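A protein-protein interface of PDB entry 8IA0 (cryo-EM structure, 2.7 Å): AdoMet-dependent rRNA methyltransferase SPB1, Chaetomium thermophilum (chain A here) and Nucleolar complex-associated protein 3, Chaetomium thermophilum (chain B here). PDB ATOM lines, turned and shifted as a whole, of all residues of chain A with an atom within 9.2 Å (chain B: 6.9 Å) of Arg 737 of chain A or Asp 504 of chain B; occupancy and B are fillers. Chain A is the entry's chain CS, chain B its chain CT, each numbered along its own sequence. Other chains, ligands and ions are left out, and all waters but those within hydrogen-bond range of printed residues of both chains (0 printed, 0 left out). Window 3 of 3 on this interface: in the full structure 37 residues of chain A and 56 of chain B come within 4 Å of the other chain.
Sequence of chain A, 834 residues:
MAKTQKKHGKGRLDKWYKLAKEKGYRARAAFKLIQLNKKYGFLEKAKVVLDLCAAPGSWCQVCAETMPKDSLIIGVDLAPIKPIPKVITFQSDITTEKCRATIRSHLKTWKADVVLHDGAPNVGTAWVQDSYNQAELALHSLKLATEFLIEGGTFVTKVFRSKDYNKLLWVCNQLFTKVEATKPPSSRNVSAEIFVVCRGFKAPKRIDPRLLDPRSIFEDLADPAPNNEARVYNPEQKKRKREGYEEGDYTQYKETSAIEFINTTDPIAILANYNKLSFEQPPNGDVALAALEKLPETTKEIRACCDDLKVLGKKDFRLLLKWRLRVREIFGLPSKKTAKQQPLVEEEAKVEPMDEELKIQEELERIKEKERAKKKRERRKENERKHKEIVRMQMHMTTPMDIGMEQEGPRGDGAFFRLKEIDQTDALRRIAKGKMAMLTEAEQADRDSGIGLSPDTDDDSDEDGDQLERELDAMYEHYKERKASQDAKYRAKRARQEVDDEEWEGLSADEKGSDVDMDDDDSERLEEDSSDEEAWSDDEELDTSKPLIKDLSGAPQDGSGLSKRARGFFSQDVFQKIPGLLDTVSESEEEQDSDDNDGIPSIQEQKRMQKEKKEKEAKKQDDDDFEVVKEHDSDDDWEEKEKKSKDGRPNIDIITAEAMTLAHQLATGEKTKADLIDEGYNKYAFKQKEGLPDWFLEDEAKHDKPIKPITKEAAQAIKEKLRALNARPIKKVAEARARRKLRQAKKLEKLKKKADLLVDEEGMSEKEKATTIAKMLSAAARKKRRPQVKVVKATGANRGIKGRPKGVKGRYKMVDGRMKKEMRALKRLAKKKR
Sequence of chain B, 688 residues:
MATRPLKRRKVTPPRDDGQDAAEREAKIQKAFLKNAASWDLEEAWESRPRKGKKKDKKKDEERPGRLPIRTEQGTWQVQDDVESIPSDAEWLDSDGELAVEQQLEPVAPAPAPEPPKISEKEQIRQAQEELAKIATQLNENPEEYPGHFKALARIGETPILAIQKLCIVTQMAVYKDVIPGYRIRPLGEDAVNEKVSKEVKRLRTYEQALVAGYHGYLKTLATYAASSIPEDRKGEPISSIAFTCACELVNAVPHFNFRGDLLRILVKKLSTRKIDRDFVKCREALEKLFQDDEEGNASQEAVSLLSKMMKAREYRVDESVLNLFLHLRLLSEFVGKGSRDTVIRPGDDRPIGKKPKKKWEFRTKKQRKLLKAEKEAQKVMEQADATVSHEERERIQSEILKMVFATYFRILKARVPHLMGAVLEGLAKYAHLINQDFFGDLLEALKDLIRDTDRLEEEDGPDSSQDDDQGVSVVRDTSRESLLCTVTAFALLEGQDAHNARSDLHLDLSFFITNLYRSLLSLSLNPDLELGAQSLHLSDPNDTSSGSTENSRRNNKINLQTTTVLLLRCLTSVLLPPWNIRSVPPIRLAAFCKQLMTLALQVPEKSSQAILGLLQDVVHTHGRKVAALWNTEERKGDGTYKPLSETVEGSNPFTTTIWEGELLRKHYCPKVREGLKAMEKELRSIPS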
ATOM      1  N   ARG A 728      -7.110  -3.921 -12.398  1.00  0.00           N
ATOM      2  CA  ARG A 728      -8.002  -2.837 -11.987  1.00  0.00           C
ATOM      3  C   ARG A 728      -7.770  -1.591 -12.833  1.00  0.00           C
ATOM      4  O   ARG A 728      -7.318  -0.560 -12.323  1.00  0.00           O
ATOM      5  CB  ARG A 728      -7.801  -2.497 -10.511  1.00  0.00           C
ATOM      6  CG  ARG A 728      -7.809  -3.671  -9.566  1.00  0.00           C
ATOM      7  CD  ARG A 728      -7.695  -3.200  -8.127  1.00  0.00           C
ATOM      8  NE  ARG A 728      -8.747  -2.256  -7.774  1.00  0.00           N
ATOM      9  CZ  ARG A 728      -8.550  -0.967  -7.532  1.00  0.00           C
ATOM     10  NH1 ARG A 728      -7.345  -0.429  -7.600  1.00  0.00           N
ATOM     11  NH2 ARG A 728      -9.589  -0.199  -7.220  1.00  0.00           N
ATOM     12  N   ILE A 730      -9.108   1.766 -14.980  1.00  0.00           N
ATOM     13  CA  ILE A 730     -10.151   2.743 -14.686  1.00  0.00           C
ATOM     14  C   ILE A 730     -11.481   2.293 -15.275  1.00  0.00           C
ATOM     15  O   ILE A 730     -12.542   2.484 -14.670  1.00  0.00           O
ATOM     16  CB  ILE A 730      -9.744   4.137 -15.197  1.00  0.00           C
ATOM     17  CG1 ILE A 730      -8.369   4.522 -14.657  1.00  0.00           C
ATOM     18  CG2 ILE A 730     -10.773   5.173 -14.794  1.00  0.00           C
ATOM     19  CD1 ILE A 730      -7.903   5.882 -15.102  1.00  0.00           C
ATOM     20  N   LYS A 731     -11.444   1.681 -16.459  1.00  0.00           N
ATOM     21  CA  LYS A 731     -12.671   1.211 -17.089  1.00  0.00           C
ATOM     22  C   LYS A 731     -13.338   0.123 -16.258  1.00  0.00           C
ATOM     23  O   LYS A 731     -14.535   0.200 -15.962  1.00  0.00           O
ATOM     24  CB  LYS A 731     -12.373   0.705 -18.501  1.00  0.00           C
ATOM     25  CG  LYS A 731     -13.600   0.244 -19.263  1.00  0.00           C
ATOM     26  CD  LYS A 731     -13.439   0.459 -20.758  1.00  0.00           C
ATOM     27  CE  LYS A 731     -12.094  -0.051 -21.250  1.00  0.00           C
ATOM     28  NZ  LYS A 731     -12.221  -0.815 -22.521  1.00  0.00           N
ATOM     29  N   LYS A 732     -12.572  -0.893 -15.852  1.00  0.00           N
ATOM     30  CA  LYS A 732     -13.163  -2.048 -15.181  1.00  0.00           C
ATOM     31  C   LYS A 732     -13.760  -1.674 -13.831  1.00  0.00           C
ATOM     32  O   LYS A 732     -14.836  -2.164 -13.469  1.00  0.00           O
ATOM     33  CB  LYS A 732     -12.122  -3.153 -15.019  1.00  0.00           C
ATOM     34  CG  LYS A 732     -11.760  -3.852 -16.315  1.00  0.00           C
ATOM     35  CD  LYS A 732     -11.976  -5.350 -16.207  1.00  0.00           C
ATOM     36  CE  LYS A 732     -10.759  -6.043 -15.617  1.00  0.00           C
ATOM     37  NZ  LYS A 732      -9.682  -6.229 -16.628  1.00  0.00           N
ATOM     38  N   VAL A 733     -13.079  -0.819 -13.070  1.00  0.00           N
ATOM     39  CA  VAL A 733     -13.616  -0.386 -11.783  1.00  0.00           C
ATOM     40  C   VAL A 733     -14.894   0.417 -11.986  1.00  0.00           C
ATOM     41  O   VAL A 733     -15.837   0.325 -11.192  1.00  0.00           O
ATOM     42  CB  VAL A 733     -12.553   0.414 -11.008  1.00  0.00           C
ATOM     43  CG1 VAL A 733     -13.139   1.000  -9.734  1.00  0.00           C
ATOM     44  CG2 VAL A 733     -11.353  -0.460 -10.695  1.00  0.00           C
ATOM     45  N   ALA A 734     -14.946   1.213 -13.057  1.00  0.00           N
ATOM     46  CA  ALA A 734     -16.128   2.024 -13.326  1.00  0.00           C
ATOM     47  C   ALA A 734     -17.355   1.162 -13.595  1.00  0.00           C
ATOM     48  O   ALA A 734     -18.449   1.460 -13.103  1.00  0.00           O
ATOM     49  CB  ALA A 734     -15.862   2.959 -14.505  1.00  0.00           C
ATOM     50  N   GLU A 735     -17.199   0.092 -14.380  1.00  0.00           N
ATOM     51  CA  GLU A 735     -18.337  -0.777 -14.668  1.00  0.00           C
ATOM     52  C   GLU A 735     -18.806  -1.511 -13.419  1.00  0.00           C
ATOM     53  O   GLU A 735     -20.009  -1.735 -13.239  1.00  0.00           O
ATOM     54  CB  GLU A 735     -17.987  -1.778 -15.770  1.00  0.00           C
ATOM     55  CG  GLU A 735     -17.055  -1.254 -16.845  1.00  0.00           C
ATOM     56  CD  GLU A 735     -17.771  -0.456 -17.919  1.00  0.00           C
ATOM     57  OE1 GLU A 735     -18.598   0.414 -17.575  1.00  0.00           O
ATOM     58  OE2 GLU A 735     -17.504  -0.702 -19.114  1.00  0.00           O
ATOM     59  N   ALA A 736     -17.872  -1.905 -12.551  1.00  0.00           N
ATOM     60  CA  ALA A 736     -18.250  -2.606 -11.330  1.00  0.00           C
ATOM     61  C   ALA A 736     -19.122  -1.730 -10.441  1.00  0.00           C
ATOM     62  O   ALA A 736     -20.118  -2.201  -9.878  1.00  0.00           O
ATOM     63  CB  ALA A 736     -17.002  -3.065 -10.578  1.00  0.00           C
ATOM     64  N   ARG A 737     -18.762  -0.454 -10.297  1.00  0.00           N
ATOM     65  CA  ARG A 737     -19.607   0.469  -9.548  1.00  0.00           C
ATOM     66  C   ARG A 737     -20.941   0.686 -10.251  1.00  0.00           C
ATOM     67  O   ARG A 737     -21.992   0.744  -9.601  1.00  0.00           O
ATOM     68  CB  ARG A 737     -18.884   1.797  -9.346  1.00  0.00           C
ATOM     69  CG  ARG A 737     -17.615   1.690  -8.524  1.00  0.00           C
ATOM     70  CD  ARG A 737     -17.615   2.693  -7.384  1.00  0.00           C
ATOM     71  NE  ARG A 737     -16.766   3.843  -7.670  1.00  0.00           N
ATOM     72  CZ  ARG A 737     -16.765   4.966  -6.964  1.00  0.00           C
ATOM     73  NH1 ARG A 737     -17.557   5.126  -5.917  1.00  0.00           N
ATOM     74  NH2 ARG A 737     -15.947   5.953  -7.318  1.00  0.00           N
ATOM     75  N   ALA A 738     -20.918   0.815 -11.578  1.00  0.00           N
ATOM     76  CA  ALA A 738     -22.158   0.975 -12.328  1.00  0.00           C
ATOM     77  C   ALA A 738     -23.035  -0.264 -12.211  1.00  0.00           C
ATOM     78  O   ALA A 738     -24.261  -0.158 -12.094  1.00  0.00           O
ATOM     79  CB  ALA A 738     -21.851   1.281 -13.793  1.00  0.00           C
ATOM     80  N   ARG A 739     -22.424  -1.450 -12.249  1.00  0.00           N
ATOM     81  CA  ARG A 739     -23.183  -2.675 -12.028  1.00  0.00           C
ATOM     82  C   ARG A 739     -23.732  -2.726 -10.610  1.00  0.00           C
ATOM     83  O   ARG A 739     -24.826  -3.254 -10.377  1.00  0.00           O
ATOM     84  CB  ARG A 739     -22.308  -3.897 -12.307  1.00  0.00           C
ATOM     85  CG  ARG A 739     -22.167  -4.236 -13.779  1.00  0.00           C
ATOM     86  CD  ARG A 739     -21.641  -5.646 -13.965  1.00  0.00           C
ATOM     87  NE  ARG A 739     -20.474  -5.907 -13.132  1.00  0.00           N
ATOM     88  CZ  ARG A 739     -19.219  -5.774 -13.538  1.00  0.00           C
ATOM     89  NH1 ARG A 739     -18.928  -5.384 -14.768  1.00  0.00           N
ATOM     90  NH2 ARG A 739     -18.231  -6.040 -12.690  1.00  0.00           N
ATOM     91  N   ARG A 740     -22.979  -2.191  -9.649  1.00  0.00           N
ATOM     92  CA  ARG A 740     -23.454  -2.145  -8.270  1.00  0.00           C
ATOM     93  C   ARG A 740     -24.706  -1.289  -8.147  1.00  0.00           C
ATOM     94  O   ARG A 740     -25.709  -1.721  -7.571  1.00  0.00           O
ATOM     95  CB  ARG A 740     -22.350  -1.615  -7.357  1.00  0.00           C
ATOM     96  CG  ARG A 740     -22.550  -1.933  -5.885  1.00  0.00           C
ATOM     97  CD  ARG A 740     -21.739  -3.143  -5.444  1.00  0.00           C
ATOM     98  NE  ARG A 740     -20.320  -3.014  -5.754  1.00  0.00           N
ATOM     99  CZ  ARG A 740     -19.715  -3.619  -6.767  1.00  0.00           C
ATOM    100  NH1 ARG A 740     -20.380  -4.406  -7.597  1.00  0.00           N
ATOM    101  NH2 ARG A 740     -18.412  -3.432  -6.950  1.00  0.00           N
ATOM    102  N   LYS A 741     -24.678  -0.076  -8.701  1.00  0.00           N
ATOM    103  CA  LYS A 741     -25.806   0.834  -8.535  1.00  0.00           C
ATOM    104  C   LYS A 741     -27.073   0.276  -9.170  1.00  0.00           C
ATOM    105  O   LYS A 741     -28.180   0.516  -8.675  1.00  0.00           O
ATOM    106  CB  LYS A 741     -25.470   2.202  -9.123  1.00  0.00           C
ATOM    107  CG  LYS A 741     -24.350   2.925  -8.398  1.00  0.00           C
ATOM    108  CD  LYS A 741     -24.750   4.349  -8.049  1.00  0.00           C
ATOM    109  CE  LYS A 741     -23.741   4.998  -7.113  1.00  0.00           C
ATOM    110  NZ  LYS A 741     -22.372   4.445  -7.298  1.00  0.00           N
ATOM    111  N   LEU A 742     -26.934  -0.465 -10.270  1.00  0.00           N
ATOM    112  CA  LEU A 742     -28.100  -1.066 -10.909  1.00  0.00           C
ATOM    113  C   LEU A 742     -28.763  -2.095 -10.004  1.00  0.00           C
ATOM    114  O   LEU A 742     -29.995  -2.167  -9.935  1.00  0.00           O
ATOM    115  CB  LEU A 742     -27.699  -1.700 -12.239  1.00  0.00           C
ATOM    116  CG  LEU A 742     -28.205  -0.992 -13.495  1.00  0.00           C
ATOM    117  CD1 LEU A 742     -27.784  -1.748 -14.740  1.00  0.00           C
ATOM    118  CD2 LEU A 742     -29.713  -0.835 -13.442  1.00  0.00           C
ATOM    119  N   ARG A 743     -27.965  -2.903  -9.302  1.00  0.00           N
ATOM    120  CA  ARG A 743     -28.526  -3.986  -8.499  1.00  0.00           C
ATOM    121  C   ARG A 743     -29.378  -3.451  -7.353  1.00  0.00           C
ATOM    122  O   ARG A 743     -30.483  -3.948  -7.107  1.00  0.00           O
ATOM    123  CB  ARG A 743     -27.406  -4.889  -7.981  1.00  0.00           C
ATOM    124  CG  ARG A 743     -27.864  -6.309  -7.689  1.00  0.00           C
ATOM    125  CD  ARG A 743     -26.750  -7.222  -7.180  1.00  0.00           C
ATOM    126  NE  ARG A 743     -25.602  -6.510  -6.632  1.00  0.00           N
ATOM    127  CZ  ARG A 743     -24.505  -6.217  -7.317  1.00  0.00           C
ATOM    128  NH1 ARG A 743     -24.374  -6.558  -8.589  1.00  0.00           N
ATOM    129  NH2 ARG A 743     -23.515  -5.569  -6.712  1.00  0.00           N
ATOM    130  N   GLN A 744     -28.883  -2.440  -6.635  1.00  0.00           N
ATOM    131  CA  GLN A 744     -29.725  -1.764  -5.653  1.00  0.00           C
ATOM    132  C   GLN A 744     -30.904  -1.056  -6.305  1.00  0.00           C
ATOM    133  O   GLN A 744     -31.998  -1.029  -5.732  1.00  0.00           O
ATOM    134  CB  GLN A 744     -28.900  -0.776  -4.822  1.00  0.00           C
ATOM    135  CG  GLN A 744     -27.884  -1.370  -3.825  1.00  0.00           C
ATOM    136  CD  GLN A 744     -26.761  -2.192  -4.433  1.00  0.00           C
ATOM    137  OE1 GLN A 744     -26.884  -2.740  -5.523  1.00  0.00           O
ATOM    138  NE2 GLN A 744     -25.646  -2.275  -3.718  1.00  0.00           N
ATOM    139  N   ALA A 745     -30.706  -0.469  -7.486  1.00  0.00           N
ATOM    140  CA  ALA A 745     -31.815   0.178  -8.177  1.00  0.00           C
ATOM    141  C   ALA A 745     -32.895  -0.833  -8.542  1.00  0.00           C
ATOM    142  O   ALA A 745     -34.091  -0.572  -8.367  1.00  0.00           O
ATOM    143  CB  ALA A 745     -31.307   0.904  -9.423  1.00  0.00           C
ATOM    144  N   GLN B 436      -5.395   1.336 -11.594  1.00  0.00           N
ATOM    145  CA  GLN B 436      -5.706   2.722 -11.254  1.00  0.00           C
ATOM    146  C   GLN B 436      -4.603   3.364 -10.421  1.00  0.00           C
ATOM    147  O   GLN B 436      -4.185   4.494 -10.691  1.00  0.00           O
ATOM    148  CB  GLN B 436      -7.029   2.797 -10.492  1.00  0.00           C
ATOM    149  CG  GLN B 436      -8.266   2.631 -11.332  1.00  0.00           C
ATOM    150  CD  GLN B 436      -9.525   2.875 -10.532  1.00  0.00           C
ATOM    151  OE1 GLN B 436     -10.617   2.980 -11.086  1.00  0.00           O
ATOM    152  NE2 GLN B 436      -9.378   2.975  -9.218  1.00  0.00           N
ATOM    153  N   ASN B 500     -13.140  11.048 -16.298  1.00  0.00           N
ATOM    154  CA  ASN B 500     -14.202  10.708 -15.361  1.00  0.00           C
ATOM    155  C   ASN B 500     -13.661  10.301 -13.998  1.00  0.00           C
ATOM    156  O   ASN B 500     -14.421  10.275 -13.025  1.00  0.00           O
ATOM    157  CB  ASN B 500     -15.072   9.591 -15.936  1.00  0.00           C
ATOM    158  CG  ASN B 500     -16.030  10.092 -16.992  1.00  0.00           C
ATOM    159  OD1 ASN B 500     -15.815  11.143 -17.592  1.00  0.00           O
ATOM    160  ND2 ASN B 500     -17.099   9.340 -17.227  1.00  0.00           N
ATOM    161  N   ALA B 501     -12.370   9.987 -13.907  1.00  0.00           N
ATOM    162  CA  ALA B 501     -11.764   9.611 -12.638  1.00  0.00           C
ATOM    163  C   ALA B 501     -10.916  10.724 -12.038  1.00  0.00           C
ATOM    164  O   ALA B 501     -10.089  10.445 -11.164  1.00  0.00           O
ATOM    165  CB  ALA B 501     -10.914   8.353 -12.815  1.00  0.00           C
ATOM    166  N   ARG B 502     -11.085  11.963 -12.502  1.00  0.00           N
ATOM    167  CA  ARG B 502     -10.338  13.097 -11.971  1.00  0.00           C
ATOM    168  C   ARG B 502     -10.479  13.209 -10.458  1.00  0.00           C
ATOM    169  O   ARG B 502      -9.487  13.190  -9.721  1.00  0.00           O
ATOM    170  CB  ARG B 502     -10.815  14.387 -12.642  1.00  0.00           C
ATOM    171  CG  ARG B 502     -10.175  14.679 -13.979  1.00  0.00           C
ATOM    172  CD  ARG B 502     -11.080  15.563 -14.814  1.00  0.00           C
ATOM    173  NE  ARG B 502     -11.859  16.481 -13.994  1.00  0.00           N
ATOM    174  CZ  ARG B 502     -13.165  16.675 -14.121  1.00  0.00           C
ATOM    175  NH1 ARG B 502     -13.883  15.991 -14.996  1.00  0.00           N
ATOM    176  NH2 ARG B 502     -13.767  17.569 -13.343  1.00  0.00           N
ATOM    177  N   SER B 503     -11.719  13.337  -9.984  1.00  0.00           N
ATOM    178  CA  SER B 503     -11.950  13.520  -8.555  1.00  0.00           C
ATOM    179  C   SER B 503     -11.538  12.291  -7.756  1.00  0.00           C
ATOM    180  O   SER B 503     -10.943  12.414  -6.681  1.00  0.00           O
ATOM    181  CB  SER B 503     -13.419  13.854  -8.304  1.00  0.00           C
ATOM    182  OG  SER B 503     -13.792  15.033  -8.993  1.00  0.00           O
ATOM    183  N   ASP B 504     -11.851  11.098  -8.263  1.00  0.00           N
ATOM    184  CA  ASP B 504     -11.601   9.882  -7.497  1.00  0.00           C
ATOM    185  C   ASP B 504     -10.110   9.619  -7.325  1.00  0.00           C
ATOM    186  O   ASP B 504      -9.660   9.276  -6.226  1.00  0.00           O
ATOM    187  CB  ASP B 504     -12.284   8.695  -8.170  1.00  0.00           C
ATOM    188  CG  ASP B 504     -13.766   8.922  -8.382  1.00  0.00           C
ATOM    189  OD1 ASP B 504     -14.123   9.867  -9.116  1.00  0.00           O
ATOM    190  OD2 ASP B 504     -14.576   8.159  -7.815  1.00  0.00           O
ATOM    191  N   LEU B 505      -9.327   9.782  -8.388  1.00  0.00           N
ATOM    192  CA  LEU B 505      -7.918   9.411  -8.376  1.00  0.00           C
ATOM    193  C   LEU B 505      -6.982  10.576  -8.078  1.00  0.00           C
ATOM    194  O   LEU B 505      -5.762  10.386  -8.106  1.00  0.00           O
ATOM    195  CB  LEU B 505      -7.524   8.761  -9.708  1.00  0.00           C
ATOM    196  CG  LEU B 505      -7.907   7.307 -10.018  1.00  0.00           C
ATOM    197  CD1 LEU B 505      -9.375   6.991  -9.783  1.00  0.00           C
ATOM    198  CD2 LEU B 505      -7.511   6.963 -11.444  1.00  0.00           C
ATOM    199  N   HIS B 506      -7.514  11.765  -7.793  1.00  0.00           N
ATOM    200  CA  HIS B 506      -6.716  12.927  -7.402  1.00  0.00           C
ATOM    201  C   HIS B 506      -5.659  13.256  -8.458  1.00  0.00           C
ATOM    202  O   HIS B 506      -4.456  13.261  -8.195  1.00  0.00           O
ATOM    203  CB  HIS B 506      -6.063  12.707  -6.033  1.00  0.00           C
ATOM    204  CG  HIS B 506      -7.039  12.553  -4.911  1.00  0.00           C
ATOM    205  ND1 HIS B 506      -7.445  11.323  -4.441  1.00  0.00           N
ATOM    206  CD2 HIS B 506      -7.681  13.474  -4.156  1.00  0.00           C
ATOM    207  CE1 HIS B 506      -8.300  11.493  -3.451  1.00  0.00           C
ATOM    208  NE2 HIS B 506      -8.461  12.789  -3.258  1.00  0.00           N
ATOM    209  N   LEU B 507      -6.130  13.527  -9.669  1.00  0.00           N
ATOM    210  CA  LEU B 507      -5.260  13.880 -10.788  1.00  0.00           C
ATOM    211  C   LEU B 507      -5.375  15.383 -11.015  1.00  0.00           C
ATOM    212  O   LEU B 507      -6.274  15.847 -11.724  1.00  0.00           O
ATOM    213  CB  LEU B 507      -5.627  13.089 -12.039  1.00  0.00           C
ATOM    214  CG  LEU B 507      -5.846  11.588 -11.847  1.00  0.00           C
ATOM    215  CD1 LEU B 507      -6.586  10.995 -13.031  1.00  0.00           C
ATOM    216  CD2 LEU B 507      -4.525  10.876 -11.632  1.00  0.00           C
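Of the 9 printed residues of chain B, 4 touch a printed residue of chain A. Printed residues of chain B that touch a printed residue of chain A: Gln 436, Ala 501, Asp 504 and Leu 505. Hydrophobic or aromatic side chains of chain B within 4 Å of the printed part of chain A: Ala 501 and Leu 505. Along chain A the printed residues that touch a printed residue of chain B span positions 728 to 737. Among the printed residues, Asp or Glu carboxylates within 4 Å of a Lys or Arg side-chain nitrogen of the other chain: Arg 737 of chain A with Asp 504 of chain B.
CA of Ile 730 of chain A touches OE1 of Gln 436 of chain B, at 3.6 Å. CB of Ala 501 of chain B touches CG2 of Ile 730 of chain A (3.7 Å). Leu 505 of chain B touches Ile 730 of chain A. Gln 436 of chain B touches Val 733 of chain A (OE1 to CB, 3.2 Å).
Arg 737 of chain A touches one residue of chain B. Asp 504 of chain B touches just one residue of chain A: Arg 737. Ala 501 of chain B touches just one residue of chain A: Ile 730 (3.7 Å). Ser 503 of chain B touches none of the printed residues of chain A. Printed residues of chain A within 4 Å of Gln 436 of chain B: Arg 728 (2.8 Å), Ile 730 (3.6 Å) and Val 733 (3.2 Å). Printed residues of chain B within 4 Å of Ile 730 of chain A: Gln 436, Ala 501 and Leu 505. Of the printed residues of chain B, Arg 728 of chain A touches Gln 436. Of the printed residues of chain B, Val 733 of chain A touches Gln 436. Of the printed residues of chain A, Leu 505 of chain B touches Ile 730 (3.8 Å). The nearest residue of chain A that does not touch Asp 504 of chain B is Val 733 of chain A (7.5 Å).
The backbone NH (N) of Gln 436 of chain B sits at hydrogen-bond distance from the backbone carbonyl oxygen (O) of Arg 728 of chain A. The guanidinium group of Arg 737 of chain A lies within salt-bridge range of the side-chain carboxylate of Asp 504 of chain B (2.6 Å).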
